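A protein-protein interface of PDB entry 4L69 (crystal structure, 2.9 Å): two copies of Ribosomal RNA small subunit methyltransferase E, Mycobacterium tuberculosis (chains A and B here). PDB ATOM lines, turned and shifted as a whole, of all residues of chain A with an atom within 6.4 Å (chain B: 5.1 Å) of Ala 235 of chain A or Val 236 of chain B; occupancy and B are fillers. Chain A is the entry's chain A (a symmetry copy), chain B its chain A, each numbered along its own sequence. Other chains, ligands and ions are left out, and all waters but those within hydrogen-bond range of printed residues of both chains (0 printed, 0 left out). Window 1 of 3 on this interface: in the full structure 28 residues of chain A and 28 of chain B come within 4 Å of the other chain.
Leu 98 of chain A touches Thr 232 of chain B. CB of Ala 102 of chain A touches CG2 of Val 236 of chain B (3.7 Å). O of Ala 235 of chain A touches CG2 of Val 236 of chain B, 3.6 Å away. Ala 235 of chain B touches Val 236 of chain A. Gly 239 of chain A touches Val 236 of chain B (CA to O, 3.5 Å). C of Gly 239 of chain A touches C of Gly 239 of chain B, at 3.9 Å. CA of Ala 240 of chain A touches O of Gly 239 of chain B, at 3.4 Å. CD2 of Leu 223 of chain B touches CZ3 of Trp 248 of chain A, 3.6 Å away. CH2 of Trp 248 of chain A touches CG1 of Val 236 of chain B, at 3.7 Å. CZ3 of Trp 248 of chain A touches CB of Ala 240 of chain B, 3.8 Å away.
The side-chain carboxylate (OE1) of Glu 101 of chain A lies within hydrogen-bond range of the side-chain hydroxyl (OG1) of Thr 232 of chain B, at 2.6 Å.
Ala 235 of chain A touches Val 236 of chain B, and with the chains exchanged Val 236 of chain A touches Ala 235 of chain B. Val 236 of chain A touches Gly 239 of chain B, and with the chains exchanged Gly 239 of chain A touches Val 236 of chain B. Gly 239 of chain A touches its own counterpart, Gly 239 of chain B. Gly 239 of chain A touches Ala 240 of chain B, and with the chains exchanged Ala 240 of chain A touches Gly 239 of chain B. Of the 13 pairs that touch across the chains among the printed residues, 7 have their exchanged pair printed and touching as well.
Of the 10 printed residues of chain B, 6 touch a printed residue of chain A. Printed residues of chain B that touch a printed residue of chain A: Leu 223, Thr 232, Ala 235, Val 236, Gly 239 and Ala 240. Hydrophobic or aromatic side chains of chain B within 4 Å of the printed part of chain A: Leu 223, Val 236 and Ala 240. Along chain B the printed residues that touch a printed residue of chain A span positions 223 to 240. Printed residues of chain A that touch a printed residue of chain B: Leu 98, Glu 101, Ala 102, Ala 235, Val 236, Gly 239, Ala 240 and Trp 248. Among the printed residues, 13 pairs touch across the chains. Among the printed residues, no Asp or Glu carboxylate lies within 4 Å of a Lys or Arg side-chain nitrogen of the other chain.
Printed residues of chain B within 4 Å of Leu 98 of chain A: Thr 232. Of the printed residues of chain B, Val 236 of chain A touches Ala 235 (3.6 Å) and Gly 239 (3.5 Å). Of the printed residues of chain B, Gly 239 of chain A touches Val 236 (3.5 Å), Gly 239 (3.9 Å) and Ala 240 (3.4 Å). Printed residues of chain A within 4 Å of Thr 232 of chain B: Leu 98 and Glu 101. The nearest printed residue of chain B that does not touch Ala 235 of chain A is Thr 232 of chain B (4.7 Å). The nearest residue of chain A that does not touch Val 236 of chain B is Val 236 of chain A (4.8 Å). The nearest printed residue of chain B that does not touch Ala 240 of chain A is Ala 240 of chain B (4.1 Å).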
ATOM      1  N   ALA A  95      21.607  -5.279  11.469  1.00  0.00           N
ATOM      2  CA  ALA A  95      21.489  -4.241  10.445  1.00  0.00           C
ATOM      3  C   ALA A  95      22.754  -4.234   9.570  1.00  0.00           C
ATOM      4  O   ALA A  95      22.670  -4.386   8.355  1.00  0.00           O
ATOM      5  CB  ALA A  95      21.298  -2.891  11.115  1.00  0.00           C
ATOM      6  N   LEU A  98      22.973  -7.689   7.433  1.00  0.00           N
ATOM      7  CA  LEU A  98      22.032  -7.728   6.310  1.00  0.00           C
ATOM      8  C   LEU A  98      22.419  -6.750   5.178  1.00  0.00           C
ATOM      9  O   LEU A  98      22.418  -7.135   4.002  1.00  0.00           O
ATOM     10  CB  LEU A  98      20.580  -7.516   6.790  1.00  0.00           C
ATOM     11  CG  LEU A  98      20.095  -8.341   8.012  1.00  0.00           C
ATOM     12  CD1 LEU A  98      18.755  -7.869   8.491  1.00  0.00           C
ATOM     13  CD2 LEU A  98      20.089  -9.836   7.744  1.00  0.00           C
ATOM     14  N   ALA A  99      22.826  -5.519   5.542  1.00  0.00           N
ATOM     15  CA  ALA A  99      23.302  -4.516   4.593  1.00  0.00           C
ATOM     16  C   ALA A  99      24.550  -5.022   3.848  1.00  0.00           C
ATOM     17  O   ALA A  99      24.672  -4.777   2.646  1.00  0.00           O
ATOM     18  CB  ALA A  99      23.613  -3.231   5.322  1.00  0.00           C
ATOM     19  N   GLU A 101      25.328  -8.264   3.293  1.00  0.00           N
ATOM     20  CA  GLU A 101      24.815  -9.272   2.361  1.00  0.00           C
ATOM     21  C   GLU A 101      24.178  -8.552   1.150  1.00  0.00           C
ATOM     22  O   GLU A 101      24.505  -8.880   0.004  1.00  0.00           O
ATOM     23  CB  GLU A 101      23.791 -10.192   3.042  1.00  0.00           C
ATOM     24  CG  GLU A 101      24.366 -11.096   4.116  1.00  0.00           C
ATOM     25  CD  GLU A 101      23.350 -11.761   5.027  1.00  0.00           C
ATOM     26  OE1 GLU A 101      22.227 -12.067   4.561  1.00  0.00           O
ATOM     27  OE2 GLU A 101      23.689 -11.999   6.208  1.00  0.00           O
ATOM     28  N   ALA A 102      23.354  -7.504   1.421  1.00  0.00           N
ATOM     29  CA  ALA A 102      22.667  -6.677   0.419  1.00  0.00           C
ATOM     30  C   ALA A 102      23.599  -5.873  -0.498  1.00  0.00           C
ATOM     31  O   ALA A 102      23.121  -5.271  -1.459  1.00  0.00           O
ATOM     32  CB  ALA A 102      21.672  -5.750   1.099  1.00  0.00           C
ATOM     33  N   LEU A 197      22.871   6.216   2.061  1.00  0.00           N
ATOM     34  CA  LEU A 197      21.572   5.933   2.691  1.00  0.00           C
ATOM     35  C   LEU A 197      21.672   6.229   4.184  1.00  0.00           C
ATOM     36  O   LEU A 197      22.538   5.664   4.858  1.00  0.00           O
ATOM     37  CB  LEU A 197      21.112   4.480   2.476  1.00  0.00           C
ATOM     38  CG  LEU A 197      21.004   3.967   1.047  1.00  0.00           C
ATOM     39  CD1 LEU A 197      20.877   2.464   1.033  1.00  0.00           C
ATOM     40  CD2 LEU A 197      19.838   4.600   0.309  1.00  0.00           C
ATOM     41  N   SER A 231      16.528  -2.920  11.331  1.00  0.00           N
ATOM     42  CA  SER A 231      17.175  -4.128  10.827  1.00  0.00           C
ATOM     43  C   SER A 231      17.115  -4.253   9.283  1.00  0.00           C
ATOM     44  O   SER A 231      18.131  -4.585   8.669  1.00  0.00           O
ATOM     45  CB  SER A 231      16.584  -5.367  11.501  1.00  0.00           C
ATOM     46  OG  SER A 231      15.188  -5.248  11.745  1.00  0.00           O
ATOM     47  N   THR A 232      15.946  -3.960   8.664  1.00  0.00           N
ATOM     48  CA  THR A 232      15.709  -4.090   7.217  1.00  0.00           C
ATOM     49  C   THR A 232      15.842  -2.848   6.326  1.00  0.00           C
ATOM     50  O   THR A 232      15.953  -3.002   5.104  1.00  0.00           O
ATOM     51  CB  THR A 232      14.348  -4.739   6.943  1.00  0.00           C
ATOM     52  OG1 THR A 232      13.381  -4.229   7.854  1.00  0.00           O
ATOM     53  CG2 THR A 232      14.399  -6.239   6.995  1.00  0.00           C
ATOM     54  N   ALA A 233      15.762  -1.641   6.895  1.00  0.00           N
ATOM     55  CA  ALA A 233      15.790  -0.390   6.132  1.00  0.00           C
ATOM     56  C   ALA A 233      16.870  -0.281   5.045  1.00  0.00           C
ATOM     57  O   ALA A 233      16.524  -0.032   3.888  1.00  0.00           O
ATOM     58  CB  ALA A 233      15.824   0.803   7.066  1.00  0.00           C
ATOM     59  N   ALA A 234      18.154  -0.514   5.394  1.00  0.00           N
ATOM     60  CA  ALA A 234      19.257  -0.440   4.428  1.00  0.00           C
ATOM     61  C   ALA A 234      19.213  -1.541   3.367  1.00  0.00           C
ATOM     62  O   ALA A 234      19.398  -1.234   2.192  1.00  0.00           O
ATOM     63  CB  ALA A 234      20.596  -0.445   5.137  1.00  0.00           C
ATOM     64  N   ALA A 235      18.944  -2.804   3.761  1.00  0.00           N
ATOM     65  CA  ALA A 235      18.861  -3.925   2.815  1.00  0.00           C
ATOM     66  C   ALA A 235      17.729  -3.762   1.775  1.00  0.00           C
ATOM     67  O   ALA A 235      17.933  -4.090   0.603  1.00  0.00           O
ATOM     68  CB  ALA A 235      18.722  -5.244   3.556  1.00  0.00           C
ATOM     69  N   VAL A 236      16.560  -3.233   2.191  1.00  0.00           N
ATOM     70  CA  VAL A 236      15.437  -3.033   1.275  1.00  0.00           C
ATOM     71  C   VAL A 236      15.755  -1.877   0.336  1.00  0.00           C
ATOM     72  O   VAL A 236      15.469  -1.971  -0.859  1.00  0.00           O
ATOM     73  CB  VAL A 236      14.079  -2.878   2.018  1.00  0.00           C
ATOM     74  CG1 VAL A 236      12.942  -2.527   1.061  1.00  0.00           C
ATOM     75  CG2 VAL A 236      13.734  -4.147   2.788  1.00  0.00           C
ATOM     76  N   ALA A 237      16.381  -0.808   0.870  1.00  0.00           N
ATOM     77  CA  ALA A 237      16.763   0.377   0.099  1.00  0.00           C
ATOM     78  C   ALA A 237      17.864   0.040  -0.880  1.00  0.00           C
ATOM     79  O   ALA A 237      17.833   0.546  -1.998  1.00  0.00           O
ATOM     80  CB  ALA A 237      17.198   1.504   1.019  1.00  0.00           C
ATOM     81  N   LEU A 238      18.798  -0.854  -0.494  1.00  0.00           N
ATOM     82  CA  LEU A 238      19.874  -1.301  -1.379  1.00  0.00           C
ATOM     83  C   LEU A 238      19.342  -2.041  -2.623  1.00  0.00           C
ATOM     84  O   LEU A 238      19.886  -1.854  -3.718  1.00  0.00           O
ATOM     85  CB  LEU A 238      20.935  -2.127  -0.631  1.00  0.00           C
ATOM     86  CG  LEU A 238      22.010  -1.290   0.069  1.00  0.00           C
ATOM     87  CD1 LEU A 238      22.685  -2.072   1.177  1.00  0.00           C
ATOM     88  CD2 LEU A 238      23.034  -0.763  -0.912  1.00  0.00           C
ATOM     89  N   GLY A 239      18.272  -2.821  -2.437  1.00  0.00           N
ATOM     90  CA  GLY A 239      17.584  -3.546  -3.496  1.00  0.00           C
ATOM     91  C   GLY A 239      16.887  -2.599  -4.449  1.00  0.00           C
ATOM     92  O   GLY A 239      16.818  -2.855  -5.651  1.00  0.00           O
ATOM     93  N   ALA A 240      16.376  -1.486  -3.919  1.00  0.00           N
ATOM     94  CA  ALA A 240      15.725  -0.446  -4.702  1.00  0.00           C
ATOM     95  C   ALA A 240      16.801   0.319  -5.490  1.00  0.00           C
ATOM     96  O   ALA A 240      16.687   0.459  -6.712  1.00  0.00           O
ATOM     97  CB  ALA A 240      14.967   0.497  -3.781  1.00  0.00           C
ATOM     98  N   TRP A 248      23.306  -2.848 -10.638  1.00  0.00           N
ATOM     99  CA  TRP A 248      22.864  -4.182 -11.042  1.00  0.00           C
ATOM    100  C   TRP A 248      22.752  -4.257 -12.575  1.00  0.00           C
ATOM    101  O   TRP A 248      22.826  -5.352 -13.147  1.00  0.00           O
ATOM    102  CB  TRP A 248      21.506  -4.520 -10.393  1.00  0.00           C
ATOM    103  CG  TRP A 248      21.523  -4.783  -8.910  1.00  0.00           C
ATOM    104  CD1 TRP A 248      22.577  -4.646  -8.053  1.00  0.00           C
ATOM    105  CD2 TRP A 248      20.418  -5.240  -8.115  1.00  0.00           C
ATOM    106  NE1 TRP A 248      22.205  -5.013  -6.780  1.00  0.00           N
ATOM    107  CE2 TRP A 248      20.881  -5.366  -6.786  1.00  0.00           C
ATOM    108  CE3 TRP A 248      19.081  -5.562  -8.398  1.00  0.00           C
ATOM    109  CZ2 TRP A 248      20.049  -5.783  -5.742  1.00  0.00           C
ATOM    110  CZ3 TRP A 248      18.261  -5.979  -7.363  1.00  0.00           C
ATOM    111  CH2 TRP A 248      18.746  -6.091  -6.056  1.00  0.00           C
ATOM    112  N   LEU B 223      20.052 -11.072  -8.566  1.00  0.00           N
ATOM    113  CA  LEU B 223      19.973  -9.810  -7.828  1.00  0.00           C
ATOM    114  C   LEU B 223      21.345  -9.152  -7.796  1.00  0.00           C
ATOM    115  O   LEU B 223      21.970  -9.046  -6.741  1.00  0.00           O
ATOM    116  CB  LEU B 223      19.432  -9.997  -6.396  1.00  0.00           C
ATOM    117  CG  LEU B 223      17.977 -10.391  -6.212  1.00  0.00           C
ATOM    118  CD1 LEU B 223      17.677 -10.584  -4.744  1.00  0.00           C
ATOM    119  CD2 LEU B 223      17.036  -9.340  -6.767  1.00  0.00           C
ATOM    120  N   THR B 232      18.449 -12.689   3.602  1.00  0.00           N
ATOM    121  CA  THR B 232      18.223 -11.430   2.872  1.00  0.00           C
ATOM    122  C   THR B 232      17.601 -11.483   1.471  1.00  0.00           C
ATOM    123  O   THR B 232      17.127 -10.445   0.992  1.00  0.00           O
ATOM    124  CB  THR B 232      19.510 -10.601   2.801  1.00  0.00           C
ATOM    125  OG1 THR B 232      20.619 -11.459   2.560  1.00  0.00           O
ATOM    126  CG2 THR B 232      19.731  -9.766   4.029  1.00  0.00           C
ATOM    127  N   ALA B 233      17.657 -12.632   0.789  1.00  0.00           N
ATOM    128  CA  ALA B 233      17.173 -12.772  -0.587  1.00  0.00           C
ATOM    129  C   ALA B 233      15.797 -12.160  -0.890  1.00  0.00           C
ATOM    130  O   ALA B 233      15.702 -11.336  -1.802  1.00  0.00           O
ATOM    131  CB  ALA B 233      17.244 -14.219  -1.031  1.00  0.00           C
ATOM    132  N   ALA B 234      14.754 -12.514  -0.108  1.00  0.00           N
ATOM    133  CA  ALA B 234      13.402 -11.980  -0.312  1.00  0.00           C
ATOM    134  C   ALA B 234      13.284 -10.485  -0.011  1.00  0.00           C
ATOM    135  O   ALA B 234      12.679  -9.771  -0.806  1.00  0.00           O
ATOM    136  CB  ALA B 234      12.386 -12.763   0.496  1.00  0.00           C
ATOM    137  N   ALA B 235      13.875 -10.006   1.105  1.00  0.00           N
ATOM    138  CA  ALA B 235      13.834  -8.583   1.470  1.00  0.00           C
ATOM    139  C   ALA B 235      14.522  -7.668   0.432  1.00  0.00           C
ATOM    140  O   ALA B 235      14.008  -6.583   0.146  1.00  0.00           O
ATOM    141  CB  ALA B 235      14.425  -8.365   2.852  1.00  0.00           C
ATOM    142  N   VAL B 236      15.657  -8.112  -0.148  1.00  0.00           N
ATOM    143  CA  VAL B 236      16.372  -7.318  -1.147  1.00  0.00           C
ATOM    144  C   VAL B 236      15.577  -7.313  -2.447  1.00  0.00           C
ATOM    145  O   VAL B 236      15.472  -6.266  -3.088  1.00  0.00           O
ATOM    146  CB  VAL B 236      17.851  -7.768  -1.323  1.00  0.00           C
ATOM    147  CG1 VAL B 236      18.540  -7.029  -2.468  1.00  0.00           C
ATOM    148  CG2 VAL B 236      18.635  -7.569  -0.032  1.00  0.00           C
ATOM    149  N   ALA B 237      14.987  -8.471  -2.809  1.00  0.00           N
ATOM    150  CA  ALA B 237      14.183  -8.626  -4.023  1.00  0.00           C
ATOM    151  C   ALA B 237      12.897  -7.840  -3.910  1.00  0.00           C
ATOM    152  O   ALA B 237      12.478  -7.250  -4.903  1.00  0.00           O
ATOM    153  CB  ALA B 237      13.886 -10.091  -4.292  1.00  0.00           C
ATOM    154  N   LEU B 238      12.303  -7.773  -2.700  1.00  0.00           N
ATOM    155  CA  LEU B 238      11.090  -6.992  -2.460  1.00  0.00           C
ATOM    156  C   LEU B 238      11.306  -5.483  -2.697  1.00  0.00           C
ATOM    157  O   LEU B 238      10.413  -4.821  -3.240  1.00  0.00           O
ATOM    158  CB  LEU B 238      10.484  -7.273  -1.074  1.00  0.00           C
ATOM    159  CG  LEU B 238       9.568  -8.501  -1.021  1.00  0.00           C
ATOM    160  CD1 LEU B 238       9.431  -9.027   0.392  1.00  0.00           C
ATOM    161  CD2 LEU B 238       8.209  -8.210  -1.617  1.00  0.00           C
ATOM    162  N   GLY B 239      12.494  -4.990  -2.331  1.00  0.00           N
ATOM    163  CA  GLY B 239      12.913  -3.610  -2.534  1.00  0.00           C
ATOM    164  C   GLY B 239      13.094  -3.300  -4.005  1.00  0.00           C
ATOM    165  O   GLY B 239      12.812  -2.188  -4.451  1.00  0.00           O
ATOM    166  N   ALA B 240      13.554  -4.289  -4.773  1.00  0.00           N
ATOM    167  CA  ALA B 240      13.732  -4.176  -6.213  1.00  0.00           C
ATOM    168  C   ALA B 240      12.346  -4.187  -6.879  1.00  0.00           C
ATOM    169  O   ALA B 240      12.032  -3.286  -7.663  1.00  0.00           O
ATOM    170  CB  ALA B 240      14.577  -5.332  -6.722  1.00  0.00           C
